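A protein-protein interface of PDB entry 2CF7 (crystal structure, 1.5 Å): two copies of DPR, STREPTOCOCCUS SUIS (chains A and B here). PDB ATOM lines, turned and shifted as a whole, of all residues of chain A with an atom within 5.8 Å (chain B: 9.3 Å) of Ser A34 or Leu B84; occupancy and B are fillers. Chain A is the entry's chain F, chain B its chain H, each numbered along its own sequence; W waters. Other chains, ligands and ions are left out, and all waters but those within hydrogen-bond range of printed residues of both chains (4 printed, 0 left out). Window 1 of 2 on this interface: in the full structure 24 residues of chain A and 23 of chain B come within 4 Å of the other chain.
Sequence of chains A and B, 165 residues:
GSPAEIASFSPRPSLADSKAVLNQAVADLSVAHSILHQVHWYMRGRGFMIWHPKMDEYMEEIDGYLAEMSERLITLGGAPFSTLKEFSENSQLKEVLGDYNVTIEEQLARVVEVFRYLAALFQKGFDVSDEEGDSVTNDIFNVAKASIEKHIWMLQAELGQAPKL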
ATOM      1  N   LEU A  29     -28.824  12.180  -0.130  1.00  0.00           N
ATOM      2  CA  LEU A  29     -27.726  11.565  -0.899  1.00  0.00           C
ATOM      3  C   LEU A  29     -27.012  12.636  -1.655  1.00  0.00           C
ATOM      4  O   LEU A  29     -25.791  12.541  -1.827  1.00  0.00           O
ATOM      5  CB  LEU A  29     -28.288  10.494  -1.866  1.00  0.00           C
ATOM      6  CG  LEU A  29     -28.779   9.212  -1.192  1.00  0.00           C
ATOM      7  CD1 LEU A  29     -29.652   8.415  -2.141  1.00  0.00           C
ATOM      8  CD2 LEU A  29     -27.607   8.358  -0.656  1.00  0.00           C
ATOM      9  N   SER A  30     -27.742  13.638  -2.140  1.00  0.00           N
ATOM     10  CA  SER A  30     -27.093  14.738  -2.855  1.00  0.00           C
ATOM     11  C   SER A  30     -26.142  15.519  -1.951  1.00  0.00           C
ATOM     12  O   SER A  30     -25.012  15.858  -2.347  1.00  0.00           O
ATOM     13  CB  SER A  30     -28.131  15.681  -3.464  1.00  0.00           C
ATOM     14  OG  SER A  30     -28.894  14.985  -4.447  1.00  0.00           O
ATOM     15  N   VAL A  31     -26.584  15.804  -0.724  1.00  0.00           N
ATOM     16  CA  VAL A  31     -25.683  16.502   0.225  1.00  0.00           C
ATOM     17  C   VAL A  31     -24.551  15.565   0.656  1.00  0.00           C
ATOM     18  O   VAL A  31     -23.381  16.010   0.771  1.00  0.00           O
ATOM     19  CB  VAL A  31     -26.485  17.054   1.399  1.00  0.00           C
ATOM     20  CG1 VAL A  31     -25.552  17.692   2.464  1.00  0.00           C
ATOM     21  CG2 VAL A  31     -27.453  18.093   0.882  1.00  0.00           C
ATOM     22  N   ALA A  32     -24.844  14.264   0.855  1.00  0.00           N
ATOM     23  CA  ALA A  32     -23.776  13.327   1.280  1.00  0.00           C
ATOM     24  C   ALA A  32     -22.707  13.282   0.182  1.00  0.00           C
ATOM     25  O   ALA A  32     -21.506  13.241   0.471  1.00  0.00           O
ATOM     26  CB  ALA A  32     -24.359  11.949   1.483  1.00  0.00           C
ATOM     27  N   HIS A  33     -23.120  13.318  -1.084  1.00  0.00           N
ATOM     28  CA  HIS A  33     -22.170  13.272  -2.188  1.00  0.00           C
ATOM     29  C   HIS A  33     -21.248  14.493  -2.112  1.00  0.00           C
ATOM     30  O   HIS A  33     -20.035  14.373  -2.280  1.00  0.00           O
ATOM     31  CB  HIS A  33     -22.921  13.203  -3.531  1.00  0.00           C
ATOM     32  CG  HIS A  33     -22.056  12.766  -4.664  1.00  0.00           C
ATOM     33  ND1 HIS A  33     -21.247  13.640  -5.349  1.00  0.00           N
ATOM     34  CD2 HIS A  33     -21.872  11.551  -5.240  1.00  0.00           C
ATOM     35  CE1 HIS A  33     -20.586  12.985  -6.290  1.00  0.00           C
ATOM     36  NE2 HIS A  33     -20.954  11.721  -6.254  1.00  0.00           N
ATOM     37  N   SER A  34     -21.833  15.652  -1.812  1.00  0.00           N
ATOM     38  CA  SER A  34     -21.063  16.894  -1.705  1.00  0.00           C
ATOM     39  C   SER A  34     -20.078  16.800  -0.561  1.00  0.00           C
ATOM     40  O   SER A  34     -18.916  17.183  -0.718  1.00  0.00           O
ATOM     41  CB  SER A  34     -22.054  18.025  -1.476  1.00  0.00           C
ATOM     42  OG  SER A  34     -21.382  19.275  -1.491  1.00  0.00           O
ATOM     43  N   ILE A  35     -20.528  16.295   0.580  1.00  0.00           N
ATOM     44  CA  ILE A  35     -19.627  16.146   1.743  1.00  0.00           C
ATOM     45  C   ILE A  35     -18.469  15.172   1.441  1.00  0.00           C
ATOM     46  O   ILE A  35     -17.289  15.445   1.748  1.00  0.00           O
ATOM     47  CB  ILE A  35     -20.413  15.666   2.990  1.00  0.00           C
ATOM     48  CG1 ILE A  35     -21.392  16.746   3.429  1.00  0.00           C
ATOM     49  CG2 ILE A  35     -19.449  15.302   4.134  1.00  0.00           C
ATOM     50  CD1 ILE A  35     -22.389  16.322   4.495  1.00  0.00           C
ATOM     51  N   LEU A  36     -18.783  14.054   0.803  1.00  0.00           N
ATOM     52  CA  LEU A  36     -17.744  13.095   0.391  1.00  0.00           C
ATOM     53  C   LEU A  36     -16.755  13.724  -0.579  1.00  0.00           C
ATOM     54  O   LEU A  36     -15.566  13.426  -0.522  1.00  0.00           O
ATOM     55  CB  LEU A  36     -18.316  11.849  -0.262  1.00  0.00           C
ATOM     56  CG  LEU A  36     -19.134  10.895   0.591  1.00  0.00           C
ATOM     57  CD1 LEU A  36     -19.892   9.929  -0.296  1.00  0.00           C
ATOM     58  CD2 LEU A  36     -18.146  10.177   1.489  1.00  0.00           C
ATOM     59  N   HIS A  37     -17.273  14.575  -1.467  1.00  0.00           N
ATOM     60  CA  HIS A  37     -16.391  15.277  -2.392  1.00  0.00           C
ATOM     61  C   HIS A  37     -15.459  16.219  -1.659  1.00  0.00           C
ATOM     62  O   HIS A  37     -14.268  16.268  -1.952  1.00  0.00           O
ATOM     63  CB  HIS A  37     -17.199  16.014  -3.437  1.00  0.00           C
ATOM     64  CG  HIS A  37     -16.596  15.916  -4.786  1.00  0.00           C
ATOM     65  ND1 HIS A  37     -17.318  16.136  -5.936  1.00  0.00           N
ATOM     66  CD2 HIS A  37     -15.359  15.558  -5.174  1.00  0.00           C
ATOM     67  CE1 HIS A  37     -16.535  15.940  -6.985  1.00  0.00           C
ATOM     68  NE2 HIS A  37     -15.335  15.601  -6.551  1.00  0.00           N
ATOM     69  N   GLN A  38     -15.975  16.938  -0.665  1.00  0.00           N
ATOM     70  CA  GLN A  38     -15.134  17.764   0.180  1.00  0.00           C
ATOM     71  C   GLN A  38     -14.045  16.955   0.870  1.00  0.00           C
ATOM     72  O   GLN A  38     -12.875  17.372   0.908  1.00  0.00           O
ATOM     73  CB  GLN A  38     -16.016  18.487   1.209  1.00  0.00           C
ATOM     74  CG  GLN A  38     -15.210  19.358   2.189  1.00  0.00           C
ATOM     75  CD  GLN A  38     -16.090  20.108   3.155  1.00  0.00           C
ATOM     76  OE1 GLN A  38     -16.291  19.679   4.318  1.00  0.00           O
ATOM     77  NE2 GLN A  38     -16.620  21.212   2.695  1.00  0.00           N
ATOM     78  N   VAL A  39     -14.413  15.813   1.456  1.00  0.00           N
ATOM     79  CA  VAL A  39     -13.415  14.981   2.135  1.00  0.00           C
ATOM     80  C   VAL A  39     -12.340  14.522   1.135  1.00  0.00           C
ATOM     81  O   VAL A  39     -11.146  14.561   1.430  1.00  0.00           O
ATOM     82  CB  VAL A  39     -14.098  13.762   2.798  1.00  0.00           C
ATOM     83  CG1 VAL A  39     -13.026  12.745   3.357  1.00  0.00           C
ATOM     84  CG2 VAL A  39     -15.015  14.218   3.926  1.00  0.00           C
ATOM     85  N   TRP A  41     -11.357  16.010  -1.659  1.00  0.00           N
ATOM     86  CA  TRP A  41     -10.507  17.120  -2.083  1.00  0.00           C
ATOM     87  C   TRP A  41      -9.581  17.642  -0.997  1.00  0.00           C
ATOM     88  O   TRP A  41      -8.429  17.950  -1.264  1.00  0.00           O
ATOM     89  CB  TRP A  41     -11.383  18.260  -2.538  1.00  0.00           C
ATOM     90  CG  TRP A  41     -12.017  18.080  -3.864  1.00  0.00           C
ATOM     91  CD1 TRP A  41     -11.508  17.418  -4.946  1.00  0.00           C
ATOM     92  CD2 TRP A  41     -13.267  18.644  -4.287  1.00  0.00           C
ATOM     93  NE1 TRP A  41     -12.397  17.497  -6.006  1.00  0.00           N
ATOM     94  CE2 TRP A  41     -13.462  18.287  -5.641  1.00  0.00           C
ATOM     95  CE3 TRP A  41     -14.233  19.419  -3.644  1.00  0.00           C
ATOM     96  CZ2 TRP A  41     -14.605  18.677  -6.359  1.00  0.00           C
ATOM     97  CZ3 TRP A  41     -15.373  19.809  -4.364  1.00  0.00           C
ATOM     98  CH2 TRP A  41     -15.542  19.433  -5.692  1.00  0.00           C
ATOM     99  N   LEU A  84     -30.135  22.423  -6.482  1.00  0.00           N
ATOM    100  CA  LEU A  84     -29.296  22.482  -5.267  1.00  0.00           C
ATOM    101  C   LEU A  84     -30.049  23.111  -4.074  1.00  0.00           C
ATOM    102  O   LEU A  84     -29.890  22.660  -2.929  1.00  0.00           O
ATOM    103  CB  LEU A  84     -27.973  23.231  -5.513  1.00  0.00           C
ATOM    104  CG  LEU A  84     -27.070  22.618  -6.582  1.00  0.00           C
ATOM    105  CD1 LEU A  84     -25.668  23.286  -6.557  1.00  0.00           C
ATOM    106  CD2 LEU A  84     -26.941  21.082  -6.518  1.00  0.00           C
ATOM    107  N   PHE A  87     -32.140  20.466  -2.532  1.00  0.00           N
ATOM    108  CA  PHE A  87     -31.354  19.486  -1.762  1.00  0.00           C
ATOM    109  C   PHE A  87     -30.906  20.052  -0.413  1.00  0.00           C
ATOM    110  O   PHE A  87     -31.049  19.399   0.658  1.00  0.00           O
ATOM    111  CB  PHE A  87     -30.106  19.020  -2.520  1.00  0.00           C
ATOM    112  CG  PHE A  87     -30.347  18.428  -3.896  1.00  0.00           C
ATOM    113  CD1 PHE A  87     -29.375  18.606  -4.889  1.00  0.00           C
ATOM    114  CD2 PHE A  87     -31.489  17.679  -4.201  1.00  0.00           C
ATOM    115  CE1 PHE A  87     -29.557  18.064  -6.137  1.00  0.00           C
ATOM    116  CE2 PHE A  87     -31.651  17.106  -5.464  1.00  0.00           C
ATOM    117  CZ  PHE A  87     -30.689  17.319  -6.443  1.00  0.00           C
ATOM    118  N   SER A  88     -30.355  21.264  -0.444  1.00  0.00           N
ATOM    119  CA  SER A  88     -29.856  21.870   0.792  1.00  0.00           C
ATOM    120  C   SER A  88     -30.965  22.038   1.796  1.00  0.00           C
ATOM    121  O   SER A  88     -30.809  21.716   2.981  1.00  0.00           O
ATOM    122  CB  SER A  88     -29.265  23.240   0.515  1.00  0.00           C
ATOM    123  OG  SER A  88     -28.059  23.097  -0.150  1.00  0.00           O
ATOM    124  N   GLU A  95     -23.574  21.075   6.006  1.00  0.00           N
ATOM    125  CA  GLU A  95     -22.283  21.290   5.363  1.00  0.00           C
ATOM    126  C   GLU A  95     -21.525  22.453   5.987  1.00  0.00           C
ATOM    127  O   GLU A  95     -22.117  23.433   6.450  1.00  0.00           O
ATOM    128  CB  GLU A  95     -22.508  21.579   3.901  1.00  0.00           C
ATOM    129  CG  GLU A  95     -23.152  20.414   3.133  1.00  0.00           C
ATOM    130  CD  GLU A  95     -23.037  20.668   1.632  1.00  0.00           C
ATOM    131  OE1 GLU A  95     -22.122  20.075   1.000  1.00  0.00           O
ATOM    132  OE2 GLU A  95     -23.874  21.408   1.084  1.00  0.00           O
ATOM    133  N   VAL B  26     -15.694  24.913 -10.913  1.00  0.00           N
ATOM    134  CA  VAL B  26     -16.194  23.957  -9.901  1.00  0.00           C
ATOM    135  C   VAL B  26     -17.657  24.284  -9.592  1.00  0.00           C
ATOM    136  O   VAL B  26     -18.509  23.379  -9.577  1.00  0.00           O
ATOM    137  CB  VAL B  26     -15.320  24.014  -8.643  1.00  0.00           C
ATOM    138  CG1 VAL B  26     -15.954  23.245  -7.480  1.00  0.00           C
ATOM    139  CG2 VAL B  26     -13.955  23.417  -8.973  1.00  0.00           C
ATOM    140  N   ALA B  27     -17.996  25.553  -9.325  1.00  0.00           N
ATOM    141  CA  ALA B  27     -19.382  25.931  -9.038  1.00  0.00           C
ATOM    142  C   ALA B  27     -20.305  25.679 -10.240  1.00  0.00           C
ATOM    143  O   ALA B  27     -21.362  25.046 -10.097  1.00  0.00           O
ATOM    144  CB  ALA B  27     -19.458  27.425  -8.615  1.00  0.00           C
ATOM    145  N   SER B  30     -20.880  22.034 -11.090  1.00  0.00           N
ATOM    146  CA  SER B  30     -21.753  21.394 -10.090  1.00  0.00           C
ATOM    147  C   SER B  30     -23.233  21.712 -10.378  1.00  0.00           C
ATOM    148  O   SER B  30     -24.113  20.848 -10.275  1.00  0.00           O
ATOM    149  CB  SER B  30     -21.370  21.858  -8.686  1.00  0.00           C
ATOM    150  OG  SER B  30     -20.060  21.436  -8.343  1.00  0.00           O
ATOM    151  N   VAL B  31     -23.544  22.964 -10.698  1.00  0.00           N
ATOM    152  CA  VAL B  31     -24.940  23.328 -11.028  1.00  0.00           C
ATOM    153  C   VAL B  31     -25.311  22.734 -12.385  1.00  0.00           C
ATOM    154  O   VAL B  31     -26.428  22.227 -12.542  1.00  0.00           O
ATOM    155  CB  VAL B  31     -25.136  24.872 -10.984  1.00  0.00           C
ATOM    156  CG1 VAL B  31     -26.538  25.217 -11.399  1.00  0.00           C
ATOM    157  CG2 VAL B  31     -24.894  25.365  -9.570  1.00  0.00           C
ATOM    158  N   SER B  34     -26.409  19.252 -11.852  1.00  0.00           N
ATOM    159  CA  SER B  34     -27.735  19.224 -11.247  1.00  0.00           C
ATOM    160  C   SER B  34     -28.821  19.470 -12.310  1.00  0.00           C
ATOM    161  O   SER B  34     -29.866  18.771 -12.346  1.00  0.00           O
ATOM    162  CB  SER B  34     -27.789  20.287 -10.130  1.00  0.00           C
ATOM    163  OG  SER B  34     -29.086  20.317  -9.542  1.00  0.00           O
ATOM    164  N   LEU B  66     -15.003  18.333 -13.863  1.00  0.00           N
ATOM    165  CA  LEU B  66     -14.966  18.726 -12.458  1.00  0.00           C
ATOM    166  C   LEU B  66     -13.716  18.102 -11.773  1.00  0.00           C
ATOM    167  O   LEU B  66     -13.028  18.779 -10.974  1.00  0.00           O
ATOM    168  CB  LEU B  66     -16.250  18.302 -11.743  1.00  0.00           C
ATOM    169  CG  LEU B  66     -16.243  18.631 -10.241  1.00  0.00           C
ATOM    170  CD1 LEU B  66     -15.999  20.115  -9.959  1.00  0.00           C
ATOM    171  CD2 LEU B  66     -17.541  18.196  -9.674  1.00  0.00           C
ATOM    172  N   PRO B  80     -11.091  24.439  -3.380  1.00  0.00           N
ATOM    173  CA  PRO B  80     -12.319  24.397  -4.168  1.00  0.00           C
ATOM    174  C   PRO B  80     -13.579  24.650  -3.338  1.00  0.00           C
ATOM    175  O   PRO B  80     -13.715  24.189  -2.189  1.00  0.00           O
ATOM    176  CB  PRO B  80     -12.379  22.939  -4.668  1.00  0.00           C
ATOM    177  CG  PRO B  80     -11.514  22.152  -3.700  1.00  0.00           C
ATOM    178  CD  PRO B  80     -10.404  23.137  -3.324  1.00  0.00           C
ATOM    179  N   PHE B  81     -14.527  25.346  -3.940  1.00  0.00           N
ATOM    180  CA  PHE B  81     -15.876  25.349  -3.384  1.00  0.00           C
ATOM    181  C   PHE B  81     -16.293  23.902  -3.172  1.00  0.00           C
ATOM    182  O   PHE B  81     -15.951  23.037  -3.991  1.00  0.00           O
ATOM    183  CB  PHE B  81     -16.873  26.007  -4.339  1.00  0.00           C
ATOM    184  CG  PHE B  81     -16.563  27.466  -4.662  1.00  0.00           C
ATOM    185  CD1 PHE B  81     -16.524  27.884  -5.998  1.00  0.00           C
ATOM    186  CD2 PHE B  81     -16.347  28.378  -3.651  1.00  0.00           C
ATOM    187  CE1 PHE B  81     -16.237  29.200  -6.324  1.00  0.00           C
ATOM    188  CE2 PHE B  81     -16.087  29.704  -3.964  1.00  0.00           C
ATOM    189  CZ  PHE B  81     -16.031  30.108  -5.284  1.00  0.00           C
ATOM    190  N   SER B  82     -17.010  23.633  -2.081  1.00  0.00           N
ATOM    191  CA  SER B  82     -17.250  22.228  -1.702  1.00  0.00           C
ATOM    192  C   SER B  82     -18.468  22.087  -0.839  1.00  0.00           C
ATOM    193  O   SER B  82     -18.541  21.134  -0.053  1.00  0.00           O
ATOM    194  CB  SER B  82     -15.999  21.606  -1.063  1.00  0.00           C
ATOM    195  OG  SER B  82     -15.703  22.188   0.192  1.00  0.00           O
ATOM    196  N   THR B  83     -19.434  22.982  -1.046  1.00  0.00           N
ATOM    197  CA  THR B  83     -20.717  22.900  -0.377  1.00  0.00           C
ATOM    198  C   THR B  83     -21.753  23.327  -1.410  1.00  0.00           C
ATOM    199  O   THR B  83     -21.454  24.111  -2.301  1.00  0.00           O
ATOM    200  CB  THR B  83     -20.791  23.849   0.844  1.00  0.00           C
ATOM    201  OG1 THR B  83     -20.585  25.205   0.417  1.00  0.00           O
ATOM    202  CG2 THR B  83     -19.732  23.490   1.925  1.00  0.00           C
ATOM    203  N   LEU B  84     -22.985  22.825  -1.269  1.00  0.00           N
ATOM    204  CA  LEU B  84     -24.023  23.251  -2.218  1.00  0.00           C
ATOM    205  C   LEU B  84     -24.282  24.757  -2.183  1.00  0.00           C
ATOM    206  O   LEU B  84     -24.512  25.373  -3.208  1.00  0.00           O
ATOM    207  CB  LEU B  84     -25.320  22.475  -1.970  1.00  0.00           C
ATOM    208  CG  LEU B  84     -25.212  20.947  -2.145  1.00  0.00           C
ATOM    209  CD1 LEU B  84     -26.644  20.325  -2.176  1.00  0.00           C
ATOM    210  CD2 LEU B  84     -24.388  20.482  -3.345  1.00  0.00           C
ATOM    211  N   LYS B  85     -24.165  25.369  -1.008  1.00  0.00           N
ATOM    212  CA  LYS B  85     -24.407  26.804  -0.904  1.00  0.00           C
ATOM    213  C   LYS B  85     -23.339  27.529  -1.720  1.00  0.00           C
ATOM    214  O   LYS B  85     -23.650  28.469  -2.477  1.00  0.00           O
ATOM    215  CB  LYS B  85     -24.372  27.245   0.561  1.00  0.00           C
ATOM    216  CG  LYS B  85     -24.472  28.755   0.760  1.00  0.00           C
ATOM    217  CD  LYS B  85     -24.383  29.077   2.255  1.00  0.00           C
ATOM    218  CE  LYS B  85     -24.509  30.581   2.503  1.00  0.00           C
ATOM    219  NZ  LYS B  85     -23.200  31.273   2.367  1.00  0.00           N
ATOM    220  N   GLU B  86     -22.085  27.095  -1.621  1.00  0.00           N
ATOM    221  CA  GLU B  86     -21.071  27.775  -2.415  1.00  0.00           C
ATOM    222  C   GLU B  86     -21.319  27.608  -3.913  1.00  0.00           C
ATOM    223  O   GLU B  86     -21.087  28.511  -4.716  1.00  0.00           O
ATOM    224  CB  GLU B  86     -19.664  27.292  -2.083  1.00  0.00           C
ATOM    225  CG  GLU B  86     -19.155  27.768  -0.709  1.00  0.00           C
ATOM    226  CD  GLU B  86     -17.861  27.074  -0.345  1.00  0.00           C
ATOM    227  OE1 GLU B  86     -16.808  27.756  -0.309  1.00  0.00           O
ATOM    228  OE2 GLU B  86     -17.879  25.836  -0.136  1.00  0.00           O
ATOM    229  N   PHE B  87     -21.713  26.405  -4.311  1.00  0.00           N
ATOM    230  CA  PHE B  87     -21.922  26.188  -5.748  1.00  0.00           C
ATOM    231  C   PHE B  87     -23.035  27.072  -6.267  1.00  0.00           C
ATOM    232  O   PHE B  87     -22.895  27.691  -7.306  1.00  0.00           O
ATOM    233  CB  PHE B  87     -22.330  24.732  -5.999  1.00  0.00           C
ATOM    234  CG  PHE B  87     -21.301  23.689  -5.586  1.00  0.00           C
ATOM    235  CD1 PHE B  87     -21.740  22.402  -5.238  1.00  0.00           C
ATOM    236  CD2 PHE B  87     -19.926  23.959  -5.576  1.00  0.00           C
ATOM    237  CE1 PHE B  87     -20.826  21.422  -4.881  1.00  0.00           C
ATOM    238  CE2 PHE B  87     -18.995  22.964  -5.235  1.00  0.00           C
ATOM    239  CZ  PHE B  87     -19.457  21.675  -4.868  1.00  0.00           C
ATOM    240  N   SER B  88     -24.154  27.082  -5.548  1.00  0.00           N
ATOM    241  CA  SER B  88     -25.334  27.794  -6.000  1.00  0.00           C
ATOM    242  C   SER B  88     -25.080  29.306  -6.009  1.00  0.00           C
ATOM    243  O   SER B  88     -25.502  29.987  -6.966  1.00  0.00           O
ATOM    244  CB  SER B  88     -26.542  27.394  -5.141  1.00  0.00           C
ATOM    245  OG  SER B  88     -27.735  27.964  -5.649  1.00  0.00           O
ATOM    246  N   GLU B  89     -24.380  29.811  -4.989  1.00  0.00           N
ATOM    247  CA  GLU B  89     -24.147  31.260  -4.873  1.00  0.00           C
ATOM    248  C   GLU B  89     -23.126  31.757  -5.878  1.00  0.00           C
ATOM    249  O   GLU B  89     -23.227  32.889  -6.338  1.00  0.00           O
ATOM    250  CB  GLU B  89     -23.795  31.663  -3.443  1.00  0.00           C
ATOM    251  CG  GLU B  89     -24.961  31.368  -2.502  1.00  0.00           C
ATOM    252  CD  GLU B  89     -24.722  31.858  -1.094  1.00  0.00           C
ATOM    253  OE1 GLU B  89     -25.729  32.066  -0.371  1.00  0.00           O
ATOM    254  OE2 GLU B  89     -23.548  32.041  -0.716  1.00  0.00           O
ATOM    255  N   ASN B  90     -22.136  30.933  -6.217  1.00  0.00           N
ATOM    256  CA  ASN B  90     -21.108  31.361  -7.153  1.00  0.00           C
ATOM    257  C   ASN B  90     -21.421  31.087  -8.605  1.00  0.00           C
ATOM    258  O   ASN B  90     -20.892  31.748  -9.499  1.00  0.00           O
ATOM    259  CB  ASN B  90     -19.771  30.702  -6.808  1.00  0.00           C
ATOM    260  CG  ASN B  90     -19.129  31.322  -5.632  1.00  0.00           C
ATOM    261  OD1 ASN B  90     -18.406  32.337  -5.795  1.00  0.00           O
ATOM    262  ND2 ASN B  90     -19.434  30.820  -4.443  1.00  0.00           N
ATOM    263  N   SER B  91     -22.286  30.093  -8.862  1.00  0.00           N
ATOM    264  CA  SER B  91     -22.545  29.717 -10.264  1.00  0.00           C
ATOM    265  C   SER B  91     -23.384  30.804 -10.922  1.00  0.00           C
ATOM    266  O   SER B  91     -24.207  31.436 -10.250  1.00  0.00           O
ATOM    267  CB  SER B  91     -23.303  28.419 -10.326  1.00  0.00           C
ATOM    268  OG  SER B  91     -23.674  28.164 -11.671  1.00  0.00           O
ATOM    269  N   GLU B  95     -31.268  27.666 -11.718  1.00  0.00           N
ATOM    270  CA  GLU B  95     -32.077  26.443 -11.663  1.00  0.00           C
ATOM    271  C   GLU B  95     -33.555  26.753 -11.433  1.00  0.00           C
ATOM    272  O   GLU B  95     -33.906  27.753 -10.794  1.00  0.00           O
ATOM    273  CB  GLU B  95     -31.569  25.535 -10.534  1.00  0.00           C
ATOM    274  CG  GLU B  95     -30.116  25.036 -10.720  1.00  0.00           C
ATOM    275  CD  GLU B  95     -29.786  23.948  -9.719  1.00  0.00           C
ATOM    276  OE1 GLU B  95     -29.897  22.769 -10.110  1.00  0.00           O
ATOM    277  OE2 GLU B  95     -29.440  24.275  -8.558  1.00  0.00           O
HETATM  278  O   HOH W   1     -18.880  19.248  -2.675  1.00  0.00           O
HETATM  279  O   HOH W   2     -19.715  19.589   2.037  1.00  0.00           O
HETATM  280  O   HOH W   3     -24.183  24.072   1.642  1.00  0.00           O
HETATM  281  O   HOH W   4     -31.121  25.686  -6.726  1.00  0.00           O
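Water W2 lies within hydrogen-bond range of OE1 of Glu A95 (2.7 Å) and O of Ser B82 (2.9 Å). Water W3 lies within hydrogen-bond range of OE2 of Glu A95 (2.7 Å), N of Lys B85 (3.0 Å) and N of Leu B84 (3.4 Å). Water W1 lies within hydrogen-bond range of OG of Ser A34 and O of Ser B82. Water W4 bridges the side-chain carboxylate of Glu B95 and the backbone NH of Leu A84.
Val A31 touches Leu B84, and with the chains exchanged Leu A84 touches Val B31. Ser A34 touches Leu B84, and with the chains exchanged Leu A84 touches Ser B34. Leu A84 touches Glu B95, and with the chains exchanged Glu A95 touches Leu B84. Ser A88 touches Leu B84, but with the chains exchanged Leu A84 does not touch Ser B88 (4.2 Å). Of the 19 pairs that touch across the chains among the printed residues, 8 have their exchanged pair printed and touching as well.
Of the printed residues of chain A, Leu B84 touches Val A31, Ser A34, Phe A87, Ser A88 and Glu A95. Printed residues of chain B within 4 Å of His A37: Leu B66. Of the printed residues of chain A, Phe B81 touches Trp A41. Printed residues of chain A within 4 Å of Phe B87: Leu A84 (3.7 Å). Of the printed residues of chain B, Trp A41 touches Pro B80 (3.9 Å), Phe B81 (3.3 Å) and Ser B82 (3.8 Å). The nearest printed residue of chain A that does not touch Leu B84 is Leu A84 (4.1 Å).
N of Leu A84 is in hydrogen-bond range of OE2 of Glu B95. The side-chain hydroxyl of Ser B82 sits at hydrogen-bond distance from the side-chain amide nitrogen of Gln A38 (2.8 Å). OE2 of Glu A95 sits at hydrogen-bond distance from N of Leu B84 (2.9 Å).
Among the printed residues, merely in contact across the chains: Val A31 with Leu B84 (3.9 Å), Ser A34 with Ser B82 (3.7 Å), Ser A34 with Thr B83 (3.9 Å), Ser A34 with Leu B84 (3.7 Å), His A37 with Leu B66 (3.7 Å), Gln A38 with Thr B83 (3.9 Å), Trp A41 with Pro B80 (3.9 Å), Trp A41 with Phe B81 (3.3 Å), Trp A41 with Ser B82 (3.8 Å), Leu A84 with Val B31 (3.7 Å), Leu A84 with Ser B34 (3.8 Å), Leu A84 with Phe B87 (3.7 Å), Phe A87 with Leu B84 (3.7 Å), Ser A88 with Leu B84 (3.3 Å), Glu A95 with Ser B82 (3.9 Å) and Glu A95 with Thr B83 (3.4 Å).
The side-chain hydroxyl of Thr B83 sits at hydrogen-bond distance from the side-chain carboxylate of Glu B86, 2.8 Å away. N of Ser B82 lies within hydrogen-bond range of OE2 of Glu B86 (3.1 Å). OG of Ser B34 sits at hydrogen-bond distance from OE1 of Glu B95, 2.6 Å away. The side-chain carboxylate of Glu A95 sits at hydrogen-bond distance from the side-chain hydroxyl of Ser A34, 2.7 Å away. The side-chain hydroxyl of Ser A88 sits at hydrogen-bond distance from the backbone carbonyl oxygen of Leu A84 (3.4 Å).
Hydrophobic or aromatic side chains of chain B that line the printed part of chain A: Val B31, Leu B66, Pro B80, Leu B84 and Phe B87. Along chain B the printed residues that touch a printed residue of chain A span positions 31 to 95. Printed residues of chain A that touch a printed residue of chain B: Val A31, Ser A34, His A37, Gln A38, Trp A41, Leu A84, Phe A87, Ser A88 and Glu A95. Among the printed residues, no Asp or Glu carboxylate lies within 4 Å of a Lys or Arg side-chain nitrogen of the other chain.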
